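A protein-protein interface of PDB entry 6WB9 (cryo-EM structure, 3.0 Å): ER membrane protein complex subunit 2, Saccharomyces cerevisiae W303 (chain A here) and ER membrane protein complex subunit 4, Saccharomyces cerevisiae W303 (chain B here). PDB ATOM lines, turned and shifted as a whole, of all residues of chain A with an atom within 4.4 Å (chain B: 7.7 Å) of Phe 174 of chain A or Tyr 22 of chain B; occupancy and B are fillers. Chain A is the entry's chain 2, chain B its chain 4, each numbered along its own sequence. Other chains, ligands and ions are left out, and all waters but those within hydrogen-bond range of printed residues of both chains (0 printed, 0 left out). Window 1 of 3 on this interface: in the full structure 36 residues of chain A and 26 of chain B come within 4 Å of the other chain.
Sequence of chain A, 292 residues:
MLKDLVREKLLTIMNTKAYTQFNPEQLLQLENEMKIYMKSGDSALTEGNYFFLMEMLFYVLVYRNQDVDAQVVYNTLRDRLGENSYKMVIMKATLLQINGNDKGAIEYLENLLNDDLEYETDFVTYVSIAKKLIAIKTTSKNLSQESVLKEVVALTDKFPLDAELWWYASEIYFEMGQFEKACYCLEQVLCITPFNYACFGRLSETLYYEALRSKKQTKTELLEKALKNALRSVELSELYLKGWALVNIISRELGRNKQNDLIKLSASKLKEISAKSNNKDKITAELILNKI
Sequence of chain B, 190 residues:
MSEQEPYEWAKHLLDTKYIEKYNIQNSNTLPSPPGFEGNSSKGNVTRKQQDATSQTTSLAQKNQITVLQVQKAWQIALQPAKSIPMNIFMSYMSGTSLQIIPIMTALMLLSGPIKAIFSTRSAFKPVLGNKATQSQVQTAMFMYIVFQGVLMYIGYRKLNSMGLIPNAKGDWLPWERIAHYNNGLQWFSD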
ATOM      1  N   SER A 170      18.877  20.035   6.044  1.00  0.00           N
ATOM      2  CA  SER A 170      20.009  19.221   6.477  1.00  0.00           C
ATOM      3  C   SER A 170      20.015  17.854   5.808  1.00  0.00           C
ATOM      4  O   SER A 170      21.088  17.299   5.565  1.00  0.00           O
ATOM      5  CB  SER A 170      19.993  19.050   7.993  1.00  0.00           C
ATOM      6  OG  SER A 170      18.946  18.190   8.395  1.00  0.00           O
ATOM      7  N   GLU A 171      18.837  17.309   5.491  1.00  0.00           N
ATOM      8  CA  GLU A 171      18.760  16.044   4.764  1.00  0.00           C
ATOM      9  C   GLU A 171      19.321  16.179   3.355  1.00  0.00           C
ATOM     10  O   GLU A 171      20.085  15.318   2.903  1.00  0.00           O
ATOM     11  CB  GLU A 171      17.314  15.553   4.712  1.00  0.00           C
ATOM     12  CG  GLU A 171      16.845  14.813   5.953  1.00  0.00           C
ATOM     13  CD  GLU A 171      17.243  13.349   5.948  1.00  0.00           C
ATOM     14  OE1 GLU A 171      17.693  12.855   4.894  1.00  0.00           O
ATOM     15  OE2 GLU A 171      17.104  12.690   6.999  1.00  0.00           O
ATOM     16  N   ILE A 172      18.963  17.258   2.650  1.00  0.00           N
ATOM     17  CA  ILE A 172      19.486  17.440   1.296  1.00  0.00           C
ATOM     18  C   ILE A 172      20.972  17.793   1.334  1.00  0.00           C
ATOM     19  O   ILE A 172      21.744  17.371   0.463  1.00  0.00           O
ATOM     20  CB  ILE A 172      18.668  18.491   0.526  1.00  0.00           C
ATOM     21  CG1 ILE A 172      17.183  18.167   0.586  1.00  0.00           C
ATOM     22  CG2 ILE A 172      19.040  18.482  -0.939  1.00  0.00           C
ATOM     23  CD1 ILE A 172      16.313  19.252   0.019  1.00  0.00           C
ATOM     24  N   TYR A 173      21.406  18.545   2.351  1.00  0.00           N
ATOM     25  CA  TYR A 173      22.829  18.853   2.493  1.00  0.00           C
ATOM     26  C   TYR A 173      23.648  17.616   2.843  1.00  0.00           C
ATOM     27  O   TYR A 173      24.807  17.508   2.429  1.00  0.00           O
ATOM     28  CB  TYR A 173      23.036  19.931   3.555  1.00  0.00           C
ATOM     29  CG  TYR A 173      22.668  21.331   3.123  1.00  0.00           C
ATOM     30  CD1 TYR A 173      22.959  21.783   1.846  1.00  0.00           C
ATOM     31  CD2 TYR A 173      22.038  22.205   4.000  1.00  0.00           C
ATOM     32  CE1 TYR A 173      22.629  23.064   1.454  1.00  0.00           C
ATOM     33  CE2 TYR A 173      21.697  23.480   3.614  1.00  0.00           C
ATOM     34  CZ  TYR A 173      21.996  23.903   2.341  1.00  0.00           C
ATOM     35  OH  TYR A 173      21.662  25.174   1.949  1.00  0.00           O
ATOM     36  N   PHE A 174      23.073  16.677   3.595  1.00  0.00           N
ATOM     37  CA  PHE A 174      23.761  15.429   3.894  1.00  0.00           C
ATOM     38  C   PHE A 174      23.732  14.472   2.712  1.00  0.00           C
ATOM     39  O   PHE A 174      24.612  13.613   2.599  1.00  0.00           O
ATOM     40  CB  PHE A 174      23.137  14.771   5.126  1.00  0.00           C
ATOM     41  CG  PHE A 174      23.838  13.517   5.570  1.00  0.00           C
ATOM     42  CD1 PHE A 174      25.023  13.589   6.277  1.00  0.00           C
ATOM     43  CD2 PHE A 174      23.308  12.269   5.284  1.00  0.00           C
ATOM     44  CE1 PHE A 174      25.669  12.445   6.692  1.00  0.00           C
ATOM     45  CE2 PHE A 174      23.951  11.119   5.694  1.00  0.00           C
ATOM     46  CZ  PHE A 174      25.133  11.208   6.399  1.00  0.00           C
ATOM     47  N   GLU A 175      22.733  14.591   1.830  1.00  0.00           N
ATOM     48  CA  GLU A 175      22.765  13.814   0.595  1.00  0.00           C
ATOM     49  C   GLU A 175      23.881  14.286  -0.327  1.00  0.00           C
ATOM     50  O   GLU A 175      24.418  13.493  -1.108  1.00  0.00           O
ATOM     51  CB  GLU A 175      21.416  13.883  -0.117  1.00  0.00           C
ATOM     52  CG  GLU A 175      20.340  13.038   0.535  1.00  0.00           C
ATOM     53  CD  GLU A 175      20.744  11.583   0.665  1.00  0.00           C
ATOM     54  OE1 GLU A 175      21.219  11.002  -0.333  1.00  0.00           O
ATOM     55  OE2 GLU A 175      20.590  11.020   1.771  1.00  0.00           O
ATOM     56  N   MET A 176      24.239  15.562  -0.248  1.00  0.00           N
ATOM     57  CA  MET A 176      25.448  16.073  -0.867  1.00  0.00           C
ATOM     58  C   MET A 176      26.607  15.909   0.115  1.00  0.00           C
ATOM     59  O   MET A 176      26.453  15.351   1.203  1.00  0.00           O
ATOM     60  CB  MET A 176      25.255  17.532  -1.271  1.00  0.00           C
ATOM     61  CG  MET A 176      23.968  17.806  -2.019  1.00  0.00           C
ATOM     62  SD  MET A 176      23.729  19.561  -2.324  1.00  0.00           S
ATOM     63  CE  MET A 176      22.410  19.502  -3.525  1.00  0.00           C
ATOM     64  N   PHE A 179      28.539  19.029   4.462  1.00  0.00           N
ATOM     65  CA  PHE A 179      28.343  18.628   5.847  1.00  0.00           C
ATOM     66  C   PHE A 179      28.279  19.818   6.796  1.00  0.00           C
ATOM     67  O   PHE A 179      27.619  19.732   7.835  1.00  0.00           O
ATOM     68  CB  PHE A 179      29.455  17.671   6.270  1.00  0.00           C
ATOM     69  CG  PHE A 179      29.391  16.335   5.592  1.00  0.00           C
ATOM     70  CD1 PHE A 179      28.188  15.659   5.475  1.00  0.00           C
ATOM     71  CD2 PHE A 179      30.534  15.758   5.065  1.00  0.00           C
ATOM     72  CE1 PHE A 179      28.128  14.430   4.851  1.00  0.00           C
ATOM     73  CE2 PHE A 179      30.479  14.528   4.439  1.00  0.00           C
ATOM     74  CZ  PHE A 179      29.274  13.864   4.333  1.00  0.00           C
ATOM     75  N   ALA A 182      24.772  21.224   6.615  1.00  0.00           N
ATOM     76  CA  ALA A 182      23.920  20.263   7.303  1.00  0.00           C
ATOM     77  C   ALA A 182      24.044  20.396   8.812  1.00  0.00           C
ATOM     78  O   ALA A 182      23.037  20.369   9.527  1.00  0.00           O
ATOM     79  CB  ALA A 182      24.273  18.842   6.869  1.00  0.00           C
ATOM     80  N   ARG A 202      21.827  12.898  14.891  1.00  0.00           N
ATOM     81  CA  ARG A 202      22.070  13.228  13.490  1.00  0.00           C
ATOM     82  C   ARG A 202      23.219  14.218  13.340  1.00  0.00           C
ATOM     83  O   ARG A 202      24.000  14.124  12.388  1.00  0.00           O
ATOM     84  CB  ARG A 202      20.797  13.783  12.857  1.00  0.00           C
ATOM     85  CG  ARG A 202      20.883  13.988  11.362  1.00  0.00           C
ATOM     86  CD  ARG A 202      21.065  12.676  10.629  1.00  0.00           C
ATOM     87  NE  ARG A 202      21.321  12.890   9.209  1.00  0.00           N
ATOM     88  CZ  ARG A 202      20.371  13.057   8.296  1.00  0.00           C
ATOM     89  NH1 ARG A 202      20.698  13.250   7.029  1.00  0.00           N
ATOM     90  NH2 ARG A 202      19.093  13.032   8.648  1.00  0.00           N
ATOM     91  N   THR A 206      26.610  13.542  11.275  1.00  0.00           N
ATOM     92  CA  THR A 206      27.147  14.421  10.238  1.00  0.00           C
ATOM     93  C   THR A 206      28.570  14.859  10.563  1.00  0.00           C
ATOM     94  O   THR A 206      29.414  14.945   9.663  1.00  0.00           O
ATOM     95  CB  THR A 206      26.252  15.644  10.044  1.00  0.00           C
ATOM     96  OG1 THR A 206      26.029  16.282  11.305  1.00  0.00           O
ATOM     97  CG2 THR A 206      24.929  15.245   9.442  1.00  0.00           C
ATOM     98  N   TYR A 209      30.770  11.859   9.791  1.00  0.00           N
ATOM     99  CA  TYR A 209      30.968  11.742   8.349  1.00  0.00           C
ATOM    100  C   TYR A 209      31.938  12.796   7.835  1.00  0.00           C
ATOM    101  O   TYR A 209      32.783  12.504   6.982  1.00  0.00           O
ATOM    102  CB  TYR A 209      29.629  11.857   7.622  1.00  0.00           C
ATOM    103  CG  TYR A 209      28.904  10.549   7.424  1.00  0.00           C
ATOM    104  CD1 TYR A 209      28.529  10.128   6.156  1.00  0.00           C
ATOM    105  CD2 TYR A 209      28.596   9.731   8.502  1.00  0.00           C
ATOM    106  CE1 TYR A 209      27.864   8.934   5.972  1.00  0.00           C
ATOM    107  CE2 TYR A 209      27.934   8.541   8.330  1.00  0.00           C
ATOM    108  CZ  TYR A 209      27.572   8.147   7.066  1.00  0.00           C
ATOM    109  OH  TYR A 209      26.913   6.958   6.900  1.00  0.00           O
ATOM    110  N   HIS B  12      25.673   1.994   6.954  1.00  0.00           N
ATOM    111  CA  HIS B  12      26.522   3.032   6.395  1.00  0.00           C
ATOM    112  C   HIS B  12      27.492   3.615   7.414  1.00  0.00           C
ATOM    113  O   HIS B  12      28.278   4.500   7.063  1.00  0.00           O
ATOM    114  CB  HIS B  12      25.656   4.152   5.813  1.00  0.00           C
ATOM    115  CG  HIS B  12      24.717   3.699   4.739  1.00  0.00           C
ATOM    116  ND1 HIS B  12      24.921   2.552   4.004  1.00  0.00           N
ATOM    117  CD2 HIS B  12      23.565   4.241   4.277  1.00  0.00           C
ATOM    118  CE1 HIS B  12      23.937   2.406   3.135  1.00  0.00           C
ATOM    119  NE2 HIS B  12      23.101   3.419   3.280  1.00  0.00           N
ATOM    120  N   LEU B  13      27.459   3.148   8.662  1.00  0.00           N
ATOM    121  CA  LEU B  13      28.321   3.683   9.710  1.00  0.00           C
ATOM    122  C   LEU B  13      29.530   2.810   9.997  1.00  0.00           C
ATOM    123  O   LEU B  13      30.576   3.333  10.395  1.00  0.00           O
ATOM    124  CB  LEU B  13      27.532   3.862  11.011  1.00  0.00           C
ATOM    125  CG  LEU B  13      28.039   4.901  12.010  1.00  0.00           C
ATOM    126  CD1 LEU B  13      27.641   6.296  11.567  1.00  0.00           C
ATOM    127  CD2 LEU B  13      27.517   4.608  13.402  1.00  0.00           C
ATOM    128  N   THR B  16      34.010   2.182   6.906  1.00  0.00           N
ATOM    129  CA  THR B  16      34.704   3.455   6.764  1.00  0.00           C
ATOM    130  C   THR B  16      35.037   3.783   5.316  1.00  0.00           C
ATOM    131  O   THR B  16      35.384   4.932   5.026  1.00  0.00           O
ATOM    132  CB  THR B  16      35.985   3.455   7.600  1.00  0.00           C
ATOM    133  OG1 THR B  16      36.770   2.301   7.275  1.00  0.00           O
ATOM    134  CG2 THR B  16      35.653   3.436   9.083  1.00  0.00           C
ATOM    135  N   LYS B  17      34.938   2.812   4.406  1.00  0.00           N
ATOM    136  CA  LYS B  17      35.185   3.066   2.994  1.00  0.00           C
ATOM    137  C   LYS B  17      33.976   3.663   2.286  1.00  0.00           C
ATOM    138  O   LYS B  17      34.128   4.210   1.190  1.00  0.00           O
ATOM    139  CB  LYS B  17      35.608   1.773   2.297  1.00  0.00           C
ATOM    140  CG  LYS B  17      36.731   1.032   3.006  1.00  0.00           C
ATOM    141  CD  LYS B  17      37.984   1.886   3.107  1.00  0.00           C
ATOM    142  CE  LYS B  17      38.652   2.056   1.753  1.00  0.00           C
ATOM    143  NZ  LYS B  17      39.139   0.756   1.214  1.00  0.00           N
ATOM    144  N   TYR B  18      32.786   3.573   2.889  1.00  0.00           N
ATOM    145  CA  TYR B  18      31.600   4.175   2.286  1.00  0.00           C
ATOM    146  C   TYR B  18      31.656   5.696   2.352  1.00  0.00           C
ATOM    147  O   TYR B  18      31.191   6.380   1.433  1.00  0.00           O
ATOM    148  CB  TYR B  18      30.338   3.654   2.976  1.00  0.00           C
ATOM    149  CG  TYR B  18      29.081   4.414   2.615  1.00  0.00           C
ATOM    150  CD1 TYR B  18      28.501   4.277   1.360  1.00  0.00           C
ATOM    151  CD2 TYR B  18      28.472   5.266   3.531  1.00  0.00           C
ATOM    152  CE1 TYR B  18      27.351   4.970   1.025  1.00  0.00           C
ATOM    153  CE2 TYR B  18      27.323   5.964   3.203  1.00  0.00           C
ATOM    154  CZ  TYR B  18      26.767   5.809   1.950  1.00  0.00           C
ATOM    155  OH  TYR B  18      25.623   6.499   1.621  1.00  0.00           O
ATOM    156  N   ILE B  19      32.222   6.239   3.431  1.00  0.00           N
ATOM    157  CA  ILE B  19      32.332   7.687   3.571  1.00  0.00           C
ATOM    158  C   ILE B  19      33.396   8.232   2.620  1.00  0.00           C
ATOM    159  O   ILE B  19      33.265   9.346   2.097  1.00  0.00           O
ATOM    160  CB  ILE B  19      32.601   8.043   5.048  1.00  0.00           C
ATOM    161  CG1 ILE B  19      31.464   7.519   5.930  1.00  0.00           C
ATOM    162  CG2 ILE B  19      32.709   9.546   5.258  1.00  0.00           C
ATOM    163  CD1 ILE B  19      31.820   6.316   6.775  1.00  0.00           C
ATOM    164  N   GLU B  20      34.441   7.447   2.343  1.00  0.00           N
ATOM    165  CA  GLU B  20      35.372   7.821   1.284  1.00  0.00           C
ATOM    166  C   GLU B  20      34.725   7.692  -0.091  1.00  0.00           C
ATOM    167  O   GLU B  20      35.019   8.484  -0.993  1.00  0.00           O
ATOM    168  CB  GLU B  20      36.635   6.965   1.364  1.00  0.00           C
ATOM    169  CG  GLU B  20      37.103   6.666   2.782  1.00  0.00           C
ATOM    170  CD  GLU B  20      37.477   7.911   3.564  1.00  0.00           C
ATOM    171  OE1 GLU B  20      38.061   8.842   2.970  1.00  0.00           O
ATOM    172  OE2 GLU B  20      37.186   7.956   4.776  1.00  0.00           O
ATOM    173  N   LYS B  21      33.844   6.703  -0.262  1.00  0.00           N
ATOM    174  CA  LYS B  21      33.031   6.598  -1.468  1.00  0.00           C
ATOM    175  C   LYS B  21      31.984   7.706  -1.547  1.00  0.00           C
ATOM    176  O   LYS B  21      31.559   8.068  -2.650  1.00  0.00           O
ATOM    177  CB  LYS B  21      32.366   5.215  -1.511  1.00  0.00           C
ATOM    178  CG  LYS B  21      31.690   4.835  -2.825  1.00  0.00           C
ATOM    179  CD  LYS B  21      32.692   4.692  -3.959  1.00  0.00           C
ATOM    180  CE  LYS B  21      33.585   3.480  -3.761  1.00  0.00           C
ATOM    181  NZ  LYS B  21      34.494   3.272  -4.920  1.00  0.00           N
ATOM    182  N   TYR B  22      31.578   8.259  -0.404  1.00  0.00           N
ATOM    183  CA  TYR B  22      30.590   9.333  -0.348  1.00  0.00           C
ATOM    184  C   TYR B  22      31.190  10.607  -0.929  1.00  0.00           C
ATOM    185  O   TYR B  22      32.027  11.255  -0.294  1.00  0.00           O
ATOM    186  CB  TYR B  22      30.147   9.547   1.097  1.00  0.00           C
ATOM    187  CG  TYR B  22      28.741  10.066   1.266  1.00  0.00           C
ATOM    188  CD1 TYR B  22      27.656   9.200   1.214  1.00  0.00           C
ATOM    189  CD2 TYR B  22      28.499  11.414   1.497  1.00  0.00           C
ATOM    190  CE1 TYR B  22      26.367   9.664   1.375  1.00  0.00           C
ATOM    191  CE2 TYR B  22      27.212  11.888   1.660  1.00  0.00           C
ATOM    192  CZ  TYR B  22      26.152  11.007   1.597  1.00  0.00           C
ATOM    193  OH  TYR B  22      24.866  11.463   1.759  1.00  0.00           O
ATOM    194  N   ASN B  23      30.765  10.969  -2.135  1.00  0.00           N
ATOM    195  CA  ASN B  23      31.329  12.110  -2.836  1.00  0.00           C
ATOM    196  C   ASN B  23      30.621  13.403  -2.439  1.00  0.00           C
ATOM    197  O   ASN B  23      29.638  13.407  -1.696  1.00  0.00           O
ATOM    198  CB  ASN B  23      31.251  11.900  -4.349  1.00  0.00           C
ATOM    199  CG  ASN B  23      32.332  10.969  -4.864  1.00  0.00           C
ATOM    200  OD1 ASN B  23      33.469  10.995  -4.389  1.00  0.00           O
ATOM    201  ND2 ASN B  23      31.984  10.138  -5.840  1.00  0.00           N
ATOM    202  N   ILE B  24      31.142  14.513  -2.953  1.00  0.00           N
ATOM    203  CA  ILE B  24      30.665  15.851  -2.633  1.00  0.00           C
ATOM    204  C   ILE B  24      30.087  16.473  -3.896  1.00  0.00           C
ATOM    205  O   ILE B  24      30.699  16.404  -4.968  1.00  0.00           O
ATOM    206  CB  ILE B  24      31.800  16.730  -2.059  1.00  0.00           C
ATOM    207  CG1 ILE B  24      32.490  16.025  -0.892  1.00  0.00           C
ATOM    208  CG2 ILE B  24      31.277  18.089  -1.617  1.00  0.00           C
ATOM    209  CD1 ILE B  24      33.888  15.537  -1.216  1.00  0.00           C
ATOM    210  N   GLN B  25      28.908  17.073  -3.771  1.00  0.00           N
ATOM    211  CA  GLN B  25      28.308  17.796  -4.880  1.00  0.00           C
ATOM    212  C   GLN B  25      28.903  19.196  -4.983  1.00  0.00           C
ATOM    213  O   GLN B  25      29.355  19.777  -3.993  1.00  0.00           O
ATOM    214  CB  GLN B  25      26.791  17.880  -4.710  1.00  0.00           C
ATOM    215  CG  GLN B  25      26.084  16.537  -4.780  1.00  0.00           C
ATOM    216  CD  GLN B  25      26.059  15.959  -6.179  1.00  0.00           C
ATOM    217  OE1 GLN B  25      26.932  15.181  -6.556  1.00  0.00           O
ATOM    218  NE2 GLN B  25      25.051  16.338  -6.957  1.00  0.00           N
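The side-chain hydroxyl of Tyr 209 of chain A is in hydrogen-bond range of the backbone carbonyl oxygen of His 12 of chain B, at 2.8 Å. O of Phe 174 of chain A sits close to OH of Tyr 22 of chain B (2.3 Å).
Among the printed residues, merely in contact across the chains: Glu 175 of chain A with Tyr 22 of chain B (3.4 Å), Tyr 209 of chain A with Ile 19 of chain B (3.4 Å), Met 176 of chain A with Tyr 22 of chain B (3.6 Å), Met 176 of chain A with Gln 25 of chain B (3.7 Å), Phe 179 of chain A with Tyr 22 of chain B (3.8 Å), Tyr 209 of chain A with Tyr 18 of chain B (3.9 Å) and Tyr 209 of chain A with Leu 13 of chain B (3.95 Å).
Phe 174 of chain A touches one residue of chain B. Printed residues of chain B within 4 Å of Glu 175 of chain A: Tyr 22. Of the printed residues of chain A, Leu 13 of chain B touches Tyr 209. Of chain A, only Phe 174 (2.3 Å), Glu 175 (3.4 Å), Met 176 (3.6 Å) and Phe 179 (3.8 Å) come within 4 Å of Tyr 22 of chain B. The nearest printed residue of chain B that does not touch Met 176 of chain A is Asn 23 of chain B (4.3 Å).
Hydrophobic or aromatic side chains of chain B that line the printed part of chain A: His 12, Leu 13, Tyr 18, Ile 19 and Tyr 22. Printed residues of chain A that touch a printed residue of chain B: Phe 174, Glu 175, Met 176, Phe 179 and Tyr 209. Along chain A the printed residues that touch a printed residue of chain B span positions 174 to 209.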
